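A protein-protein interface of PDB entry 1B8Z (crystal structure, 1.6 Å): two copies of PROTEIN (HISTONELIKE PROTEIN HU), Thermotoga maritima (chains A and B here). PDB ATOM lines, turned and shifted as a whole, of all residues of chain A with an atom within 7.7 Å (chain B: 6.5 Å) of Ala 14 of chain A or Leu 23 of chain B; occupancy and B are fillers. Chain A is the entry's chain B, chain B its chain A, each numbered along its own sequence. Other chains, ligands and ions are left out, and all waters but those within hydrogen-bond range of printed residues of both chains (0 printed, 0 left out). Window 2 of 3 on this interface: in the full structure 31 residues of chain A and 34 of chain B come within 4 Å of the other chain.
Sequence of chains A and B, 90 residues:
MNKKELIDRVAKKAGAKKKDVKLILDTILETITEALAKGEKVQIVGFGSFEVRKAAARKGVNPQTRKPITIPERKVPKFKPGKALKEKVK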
ATOM      1  N   ASP A   8      35.834 -13.823 -15.051  1.00  0.00           N
ATOM      2  CA  ASP A   8      35.500 -15.019 -14.252  1.00  0.00           C
ATOM      3  C   ASP A   8      34.317 -14.788 -13.339  1.00  0.00           C
ATOM      4  O   ASP A   8      33.432 -15.667 -13.217  1.00  0.00           O
ATOM      5  CB  ASP A   8      36.721 -15.338 -13.367  1.00  0.00           C
ATOM      6  CG  ASP A   8      37.874 -15.925 -14.146  1.00  0.00           C
ATOM      7  OD1 ASP A   8      37.768 -16.263 -15.334  1.00  0.00           O
ATOM      8  OD2 ASP A   8      38.958 -16.039 -13.503  1.00  0.00           O
ATOM      9  N   ARG A   9      34.198 -13.625 -12.705  1.00  0.00           N
ATOM     10  CA  ARG A   9      33.108 -13.317 -11.799  1.00  0.00           C
ATOM     11  C   ARG A   9      31.800 -13.231 -12.592  1.00  0.00           C
ATOM     12  O   ARG A   9      30.775 -13.740 -12.132  1.00  0.00           O
ATOM     13  CB  ARG A   9      33.293 -12.007 -11.044  1.00  0.00           C
ATOM     14  CG  ARG A   9      34.505 -12.031 -10.107  1.00  0.00           C
ATOM     15  CD  ARG A   9      34.483 -10.804  -9.204  1.00  0.00           C
ATOM     16  NE  ARG A   9      35.592 -10.856  -8.243  1.00  0.00           N
ATOM     17  CZ  ARG A   9      35.467 -11.285  -6.991  1.00  0.00           C
ATOM     18  NH1 ARG A   9      34.291 -11.700  -6.533  1.00  0.00           N
ATOM     19  NH2 ARG A   9      36.530 -11.296  -6.189  1.00  0.00           N
ATOM     20  N   VAL A  10      31.861 -12.545 -13.741  1.00  0.00           N
ATOM     21  CA  VAL A  10      30.613 -12.445 -14.515  1.00  0.00           C
ATOM     22  C   VAL A  10      30.192 -13.793 -15.039  1.00  0.00           C
ATOM     23  O   VAL A  10      28.976 -14.105 -15.050  1.00  0.00           O
ATOM     24  CB  VAL A  10      30.846 -11.423 -15.670  1.00  0.00           C
ATOM     25  CG1 VAL A  10      29.707 -11.481 -16.694  1.00  0.00           C
ATOM     26  CG2 VAL A  10      31.016 -10.050 -15.067  1.00  0.00           C
ATOM     27  N   ALA A  11      31.093 -14.634 -15.521  1.00  0.00           N
ATOM     28  CA  ALA A  11      30.747 -15.953 -16.057  1.00  0.00           C
ATOM     29  C   ALA A  11      30.097 -16.784 -14.941  1.00  0.00           C
ATOM     30  O   ALA A  11      29.099 -17.455 -15.244  1.00  0.00           O
ATOM     31  CB  ALA A  11      32.004 -16.667 -16.535  1.00  0.00           C
ATOM     32  N   LYS A  12      30.581 -16.658 -13.715  1.00  0.00           N
ATOM     33  CA  LYS A  12      29.971 -17.469 -12.635  1.00  0.00           C
ATOM     34  C   LYS A  12      28.577 -16.980 -12.319  1.00  0.00           C
ATOM     35  O   LYS A  12      27.591 -17.767 -12.237  1.00  0.00           O
ATOM     36  CB  LYS A  12      30.852 -17.426 -11.374  1.00  0.00           C
ATOM     37  CG  LYS A  12      30.240 -18.254 -10.232  1.00  0.00           C
ATOM     38  CD  LYS A  12      30.963 -18.025  -8.915  1.00  0.00           C
ATOM     39  CE  LYS A  12      30.342 -18.867  -7.801  1.00  0.00           C
ATOM     40  NZ  LYS A  12      31.343 -19.183  -6.743  1.00  0.00           N
ATOM     41  N   LYS A  13      28.406 -15.667 -12.217  1.00  0.00           N
ATOM     42  CA  LYS A  13      27.116 -15.090 -11.841  1.00  0.00           C
ATOM     43  C   LYS A  13      26.057 -15.332 -12.909  1.00  0.00           C
ATOM     44  O   LYS A  13      24.890 -15.602 -12.565  1.00  0.00           O
ATOM     45  CB  LYS A  13      27.193 -13.596 -11.597  1.00  0.00           C
ATOM     46  CG  LYS A  13      27.989 -13.149 -10.376  1.00  0.00           C
ATOM     47  CD  LYS A  13      27.903 -11.634 -10.330  1.00  0.00           C
ATOM     48  CE  LYS A  13      28.850 -11.015  -9.321  1.00  0.00           C
ATOM     49  NZ  LYS A  13      28.532  -9.571  -9.150  1.00  0.00           N
ATOM     50  N   ALA A  14      26.439 -15.194 -14.179  1.00  0.00           N
ATOM     51  CA  ALA A  14      25.443 -15.362 -15.231  1.00  0.00           C
ATOM     52  C   ALA A  14      25.287 -16.805 -15.656  1.00  0.00           C
ATOM     53  O   ALA A  14      24.432 -17.103 -16.497  1.00  0.00           O
ATOM     54  CB  ALA A  14      25.903 -14.539 -16.425  1.00  0.00           C
ATOM     55  N   GLY A  15      26.133 -17.714 -15.178  1.00  0.00           N
ATOM     56  CA  GLY A  15      26.068 -19.094 -15.653  1.00  0.00           C
ATOM     57  C   GLY A  15      26.421 -19.211 -17.114  1.00  0.00           C
ATOM     58  O   GLY A  15      25.844 -19.933 -17.928  1.00  0.00           O
ATOM     59  N   ALA A  16      27.416 -18.424 -17.569  1.00  0.00           N
ATOM     60  CA  ALA A  16      27.863 -18.381 -18.938  1.00  0.00           C
ATOM     61  C   ALA A  16      29.296 -18.888 -19.082  1.00  0.00           C
ATOM     62  O   ALA A  16      30.047 -18.905 -18.093  1.00  0.00           O
ATOM     63  CB  ALA A  16      27.843 -16.909 -19.387  1.00  0.00           C
ATOM     64  N   LYS A  17      29.622 -19.321 -20.281  1.00  0.00           N
ATOM     65  CA  LYS A  17      30.984 -19.780 -20.559  1.00  0.00           C
ATOM     66  C   LYS A  17      31.918 -18.573 -20.535  1.00  0.00           C
ATOM     67  O   LYS A  17      31.522 -17.535 -21.073  1.00  0.00           O
ATOM     68  CB  LYS A  17      31.033 -20.441 -21.938  1.00  0.00           C
ATOM     69  CG  LYS A  17      30.118 -21.666 -22.023  1.00  0.00           C
ATOM     70  CD  LYS A  17      30.110 -22.180 -23.454  1.00  0.00           C
ATOM     71  CE  LYS A  17      29.422 -23.533 -23.541  1.00  0.00           C
ATOM     72  NZ  LYS A  17      28.814 -23.710 -24.895  1.00  0.00           N
ATOM     73  N   VAL A  21      31.510 -14.657 -22.372  1.00  0.00           N
ATOM     74  CA  VAL A  21      31.609 -13.417 -21.595  1.00  0.00           C
ATOM     75  C   VAL A  21      32.725 -12.559 -22.182  1.00  0.00           C
ATOM     76  O   VAL A  21      32.527 -11.357 -22.358  1.00  0.00           O
ATOM     77  CB  VAL A  21      31.855 -13.690 -20.107  1.00  0.00           C
ATOM     78  CG1 VAL A  21      32.139 -12.389 -19.378  1.00  0.00           C
ATOM     79  CG2 VAL A  21      30.630 -14.399 -19.518  1.00  0.00           C
ATOM     80  N   ILE A  24      31.565 -11.005 -25.453  1.00  0.00           N
ATOM     81  CA  ILE A  24      30.583  -9.899 -25.286  1.00  0.00           C
ATOM     82  C   ILE A  24      31.213  -8.713 -24.593  1.00  0.00           C
ATOM     83  O   ILE A  24      31.015  -7.559 -25.032  1.00  0.00           O
ATOM     84  CB  ILE A  24      29.318 -10.420 -24.601  1.00  0.00           C
ATOM     85  CG1 ILE A  24      28.562 -11.301 -25.613  1.00  0.00           C
ATOM     86  CG2 ILE A  24      28.438  -9.254 -24.177  1.00  0.00           C
ATOM     87  CD1 ILE A  24      27.514 -12.193 -25.011  1.00  0.00           C
ATOM     88  N   LYS B  18      19.971 -10.832 -28.353  1.00  0.00           N
ATOM     89  CA  LYS B  18      19.888  -9.657 -27.476  1.00  0.00           C
ATOM     90  C   LYS B  18      19.663 -10.006 -26.027  1.00  0.00           C
ATOM     91  O   LYS B  18      20.244  -9.330 -25.136  1.00  0.00           O
ATOM     92  CB  LYS B  18      18.791  -8.696 -27.961  1.00  0.00           C
ATOM     93  CG  LYS B  18      19.117  -8.020 -29.269  1.00  0.00           C
ATOM     94  CD  LYS B  18      17.934  -7.217 -29.797  1.00  0.00           C
ATOM     95  CE  LYS B  18      18.197  -6.749 -31.220  1.00  0.00           C
ATOM     96  NZ  LYS B  18      17.299  -5.609 -31.574  1.00  0.00           N
ATOM     97  N   LYS B  19      18.890 -11.026 -25.650  1.00  0.00           N
ATOM     98  CA  LYS B  19      18.680 -11.340 -24.249  1.00  0.00           C
ATOM     99  C   LYS B  19      19.971 -11.781 -23.566  1.00  0.00           C
ATOM    100  O   LYS B  19      20.135 -11.493 -22.378  1.00  0.00           O
ATOM    101  CB  LYS B  19      17.566 -12.362 -24.041  1.00  0.00           C
ATOM    102  CG  LYS B  19      17.868 -13.765 -24.521  1.00  0.00           C
ATOM    103  CD  LYS B  19      16.885 -14.769 -23.925  1.00  0.00           C
ATOM    104  CE  LYS B  19      16.825 -16.034 -24.766  1.00  0.00           C
ATOM    105  NZ  LYS B  19      15.542 -16.776 -24.574  1.00  0.00           N
ATOM    106  N   ASP B  20      20.865 -12.451 -24.292  1.00  0.00           N
ATOM    107  CA  ASP B  20      22.128 -12.899 -23.723  1.00  0.00           C
ATOM    108  C   ASP B  20      23.069 -11.713 -23.507  1.00  0.00           C
ATOM    109  O   ASP B  20      23.747 -11.619 -22.476  1.00  0.00           O
ATOM    110  CB  ASP B  20      22.822 -13.935 -24.613  1.00  0.00           C
ATOM    111  CG  ASP B  20      22.032 -15.240 -24.597  1.00  0.00           C
ATOM    112  OD1 ASP B  20      21.400 -15.550 -23.574  1.00  0.00           O
ATOM    113  OD2 ASP B  20      22.100 -15.945 -25.622  1.00  0.00           O
ATOM    114  N   VAL B  21      23.075 -10.799 -24.462  1.00  0.00           N
ATOM    115  CA  VAL B  21      23.897  -9.589 -24.334  1.00  0.00           C
ATOM    116  C   VAL B  21      23.377  -8.777 -23.160  1.00  0.00           C
ATOM    117  O   VAL B  21      24.184  -8.291 -22.375  1.00  0.00           O
ATOM    118  CB  VAL B  21      23.851  -8.774 -25.634  1.00  0.00           C
ATOM    119  CG1 VAL B  21      24.525  -7.426 -25.427  1.00  0.00           C
ATOM    120  CG2 VAL B  21      24.512  -9.551 -26.769  1.00  0.00           C
ATOM    121  N   LYS B  22      22.037  -8.649 -23.011  1.00  0.00           N
ATOM    122  CA  LYS B  22      21.548  -7.869 -21.865  1.00  0.00           C
ATOM    123  C   LYS B  22      21.910  -8.506 -20.540  1.00  0.00           C
ATOM    124  O   LYS B  22      22.333  -7.781 -19.620  1.00  0.00           O
ATOM    125  CB  LYS B  22      20.009  -7.748 -21.967  1.00  0.00           C
ATOM    126  CG  LYS B  22      19.512  -6.787 -20.886  1.00  0.00           C
ATOM    127  N   LEU B  23      21.853  -9.828 -20.442  1.00  0.00           N
ATOM    128  CA  LEU B  23      22.205 -10.516 -19.209  1.00  0.00           C
ATOM    129  C   LEU B  23      23.690 -10.292 -18.880  1.00  0.00           C
ATOM    130  O   LEU B  23      24.016  -9.873 -17.761  1.00  0.00           O
ATOM    131  CB  LEU B  23      21.924 -12.014 -19.319  1.00  0.00           C
ATOM    132  CG  LEU B  23      22.478 -12.858 -18.171  1.00  0.00           C
ATOM    133  CD1 LEU B  23      21.754 -12.544 -16.874  1.00  0.00           C
ATOM    134  CD2 LEU B  23      22.387 -14.355 -18.480  1.00  0.00           C
ATOM    135  N   ILE B  24      24.521 -10.433 -19.911  1.00  0.00           N
ATOM    136  CA  ILE B  24      25.971 -10.262 -19.632  1.00  0.00           C
ATOM    137  C   ILE B  24      26.305  -8.813 -19.367  1.00  0.00           C
ATOM    138  O   ILE B  24      27.024  -8.516 -18.388  1.00  0.00           O
ATOM    139  CB  ILE B  24      26.804 -10.875 -20.772  1.00  0.00           C
ATOM    140  CG1 ILE B  24      26.837 -12.392 -20.523  1.00  0.00           C
ATOM    141  CG2 ILE B  24      28.218 -10.323 -20.736  1.00  0.00           C
ATOM    142  CD1 ILE B  24      27.283 -13.229 -21.690  1.00  0.00           C
ATOM    143  N   LEU B  25      25.711  -7.864 -20.113  1.00  0.00           N
ATOM    144  CA  LEU B  25      25.972  -6.460 -19.808  1.00  0.00           C
ATOM    145  C   LEU B  25      25.528  -6.079 -18.414  1.00  0.00           C
ATOM    146  O   LEU B  25      26.283  -5.465 -17.657  1.00  0.00           O
ATOM    147  CB  LEU B  25      25.237  -5.589 -20.848  1.00  0.00           C
ATOM    148  CG  LEU B  25      25.268  -4.090 -20.560  1.00  0.00           C
ATOM    149  CD1 LEU B  25      26.665  -3.516 -20.492  1.00  0.00           C
ATOM    150  CD2 LEU B  25      24.421  -3.335 -21.593  1.00  0.00           C
ATOM    151  N   ASP B  26      24.297  -6.492 -18.030  1.00  0.00           N
ATOM    152  CA  ASP B  26      23.819  -6.138 -16.685  1.00  0.00           C
ATOM    153  C   ASP B  26      24.716  -6.789 -15.617  1.00  0.00           C
ATOM    154  O   ASP B  26      24.964  -6.121 -14.585  1.00  0.00           O
ATOM    155  CB  ASP B  26      22.381  -6.619 -16.525  1.00  0.00           C
ATOM    156  CG  ASP B  26      21.359  -5.722 -17.192  1.00  0.00           C
ATOM    157  OD1 ASP B  26      21.695  -4.617 -17.638  1.00  0.00           O
ATOM    158  OD2 ASP B  26      20.191  -6.180 -17.241  1.00  0.00           O
ATOM    159  N   THR B  27      25.183  -7.998 -15.834  1.00  0.00           N
ATOM    160  CA  THR B  27      26.046  -8.673 -14.852  1.00  0.00           C
ATOM    161  C   THR B  27      27.403  -7.993 -14.771  1.00  0.00           C
ATOM    162  O   THR B  27      27.953  -7.828 -13.684  1.00  0.00           O
ATOM    163  CB  THR B  27      26.185 -10.151 -15.220  1.00  0.00           C
ATOM    164  OG1 THR B  27      24.860 -10.712 -15.281  1.00  0.00           O
ATOM    165  CG2 THR B  27      26.940 -10.865 -14.107  1.00  0.00           C
ATOM    166  N   ILE B  28      27.933  -7.522 -15.913  1.00  0.00           N
ATOM    167  CA  ILE B  28      29.142  -6.721 -15.851  1.00  0.00           C
ATOM    168  C   ILE B  28      28.920  -5.450 -15.045  1.00  0.00           C
ATOM    169  O   ILE B  28      29.757  -5.118 -14.191  1.00  0.00           O
ATOM    170  CB  ILE B  28      29.603  -6.347 -17.287  1.00  0.00           C
ATOM    171  CG1 ILE B  28      30.087  -7.576 -18.025  1.00  0.00           C
ATOM    172  CG2 ILE B  28      30.673  -5.246 -17.207  1.00  0.00           C
ATOM    173  CD1 ILE B  28      30.137  -7.315 -19.533  1.00  0.00           C
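The backbone carbonyl oxygen (O) of Leu 23 of chain B lies within hydrogen-bond range of the side-chain hydroxyl (OG1) of Thr 27 of chain B (2.8 Å).
CG2 of Thr 27 of chain B touches CG1 of Val 10 of chain A (3.8 Å).
CA of Ile 28 of chain B touches CG2 of Val 10 of chain A (3.9 Å).
CB of Lys 13 of chain A touches CG2 of Thr 27 of chain B, at 3.7 Å.
Leu 23 of chain B touches Ala 14 of chain A.
CD1 of Ile 24 of chain A touches CD1 of Ile 24 of chain B, 3.5 Å away.
Of the printed residues of chain B, Lys 13 of chain A touches Thr 27.
Of the printed residues of chain B, Ala 14 of chain A touches Leu 23.
Ala 16 of chain A touches none of the printed residues of chain B.
Leu 23 of chain B touches just one residue of chain A: Ala 14 (3.96 Å).
Printed residues of chain A within 4 Å of Ile 24 of chain B: Ile 24.
Of the printed residues of chain A, Thr 27 of chain B touches Val 10 (3.8 Å) and Lys 13 (3.7 Å).
Of the printed residues of chain A, Ile 28 of chain B touches Val 10.
The nearest residue of chain B that does not touch Ala 14 of chain A is Thr 27 of chain B (4.1 Å).
The nearest printed residue of chain B that does not touch Val 10 of chain A is Ile 24 of chain B (4.3 Å).
Of the 12 printed residues of chain A, 4 touch a printed residue of chain B.
Printed residues of chain A that touch a printed residue of chain B: Val 10, Lys 13, Ala 14 and Ile 24.
Hydrophobic or aromatic side chains of chain B within 4 Å of the printed part of chain A: Leu 23, Ile 24 and Ile 28.
Among the printed residues, no Asp or Glu carboxylate lies within 4 Å of a Lys or Arg side-chain nitrogen of the other chain.
Ile 24 of chain A touches its own counterpart, Ile 24 of chain B.
Of the 5 pairs that touch across the chains among the printed residues, 1 has its exchanged pair printed and touching as well.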
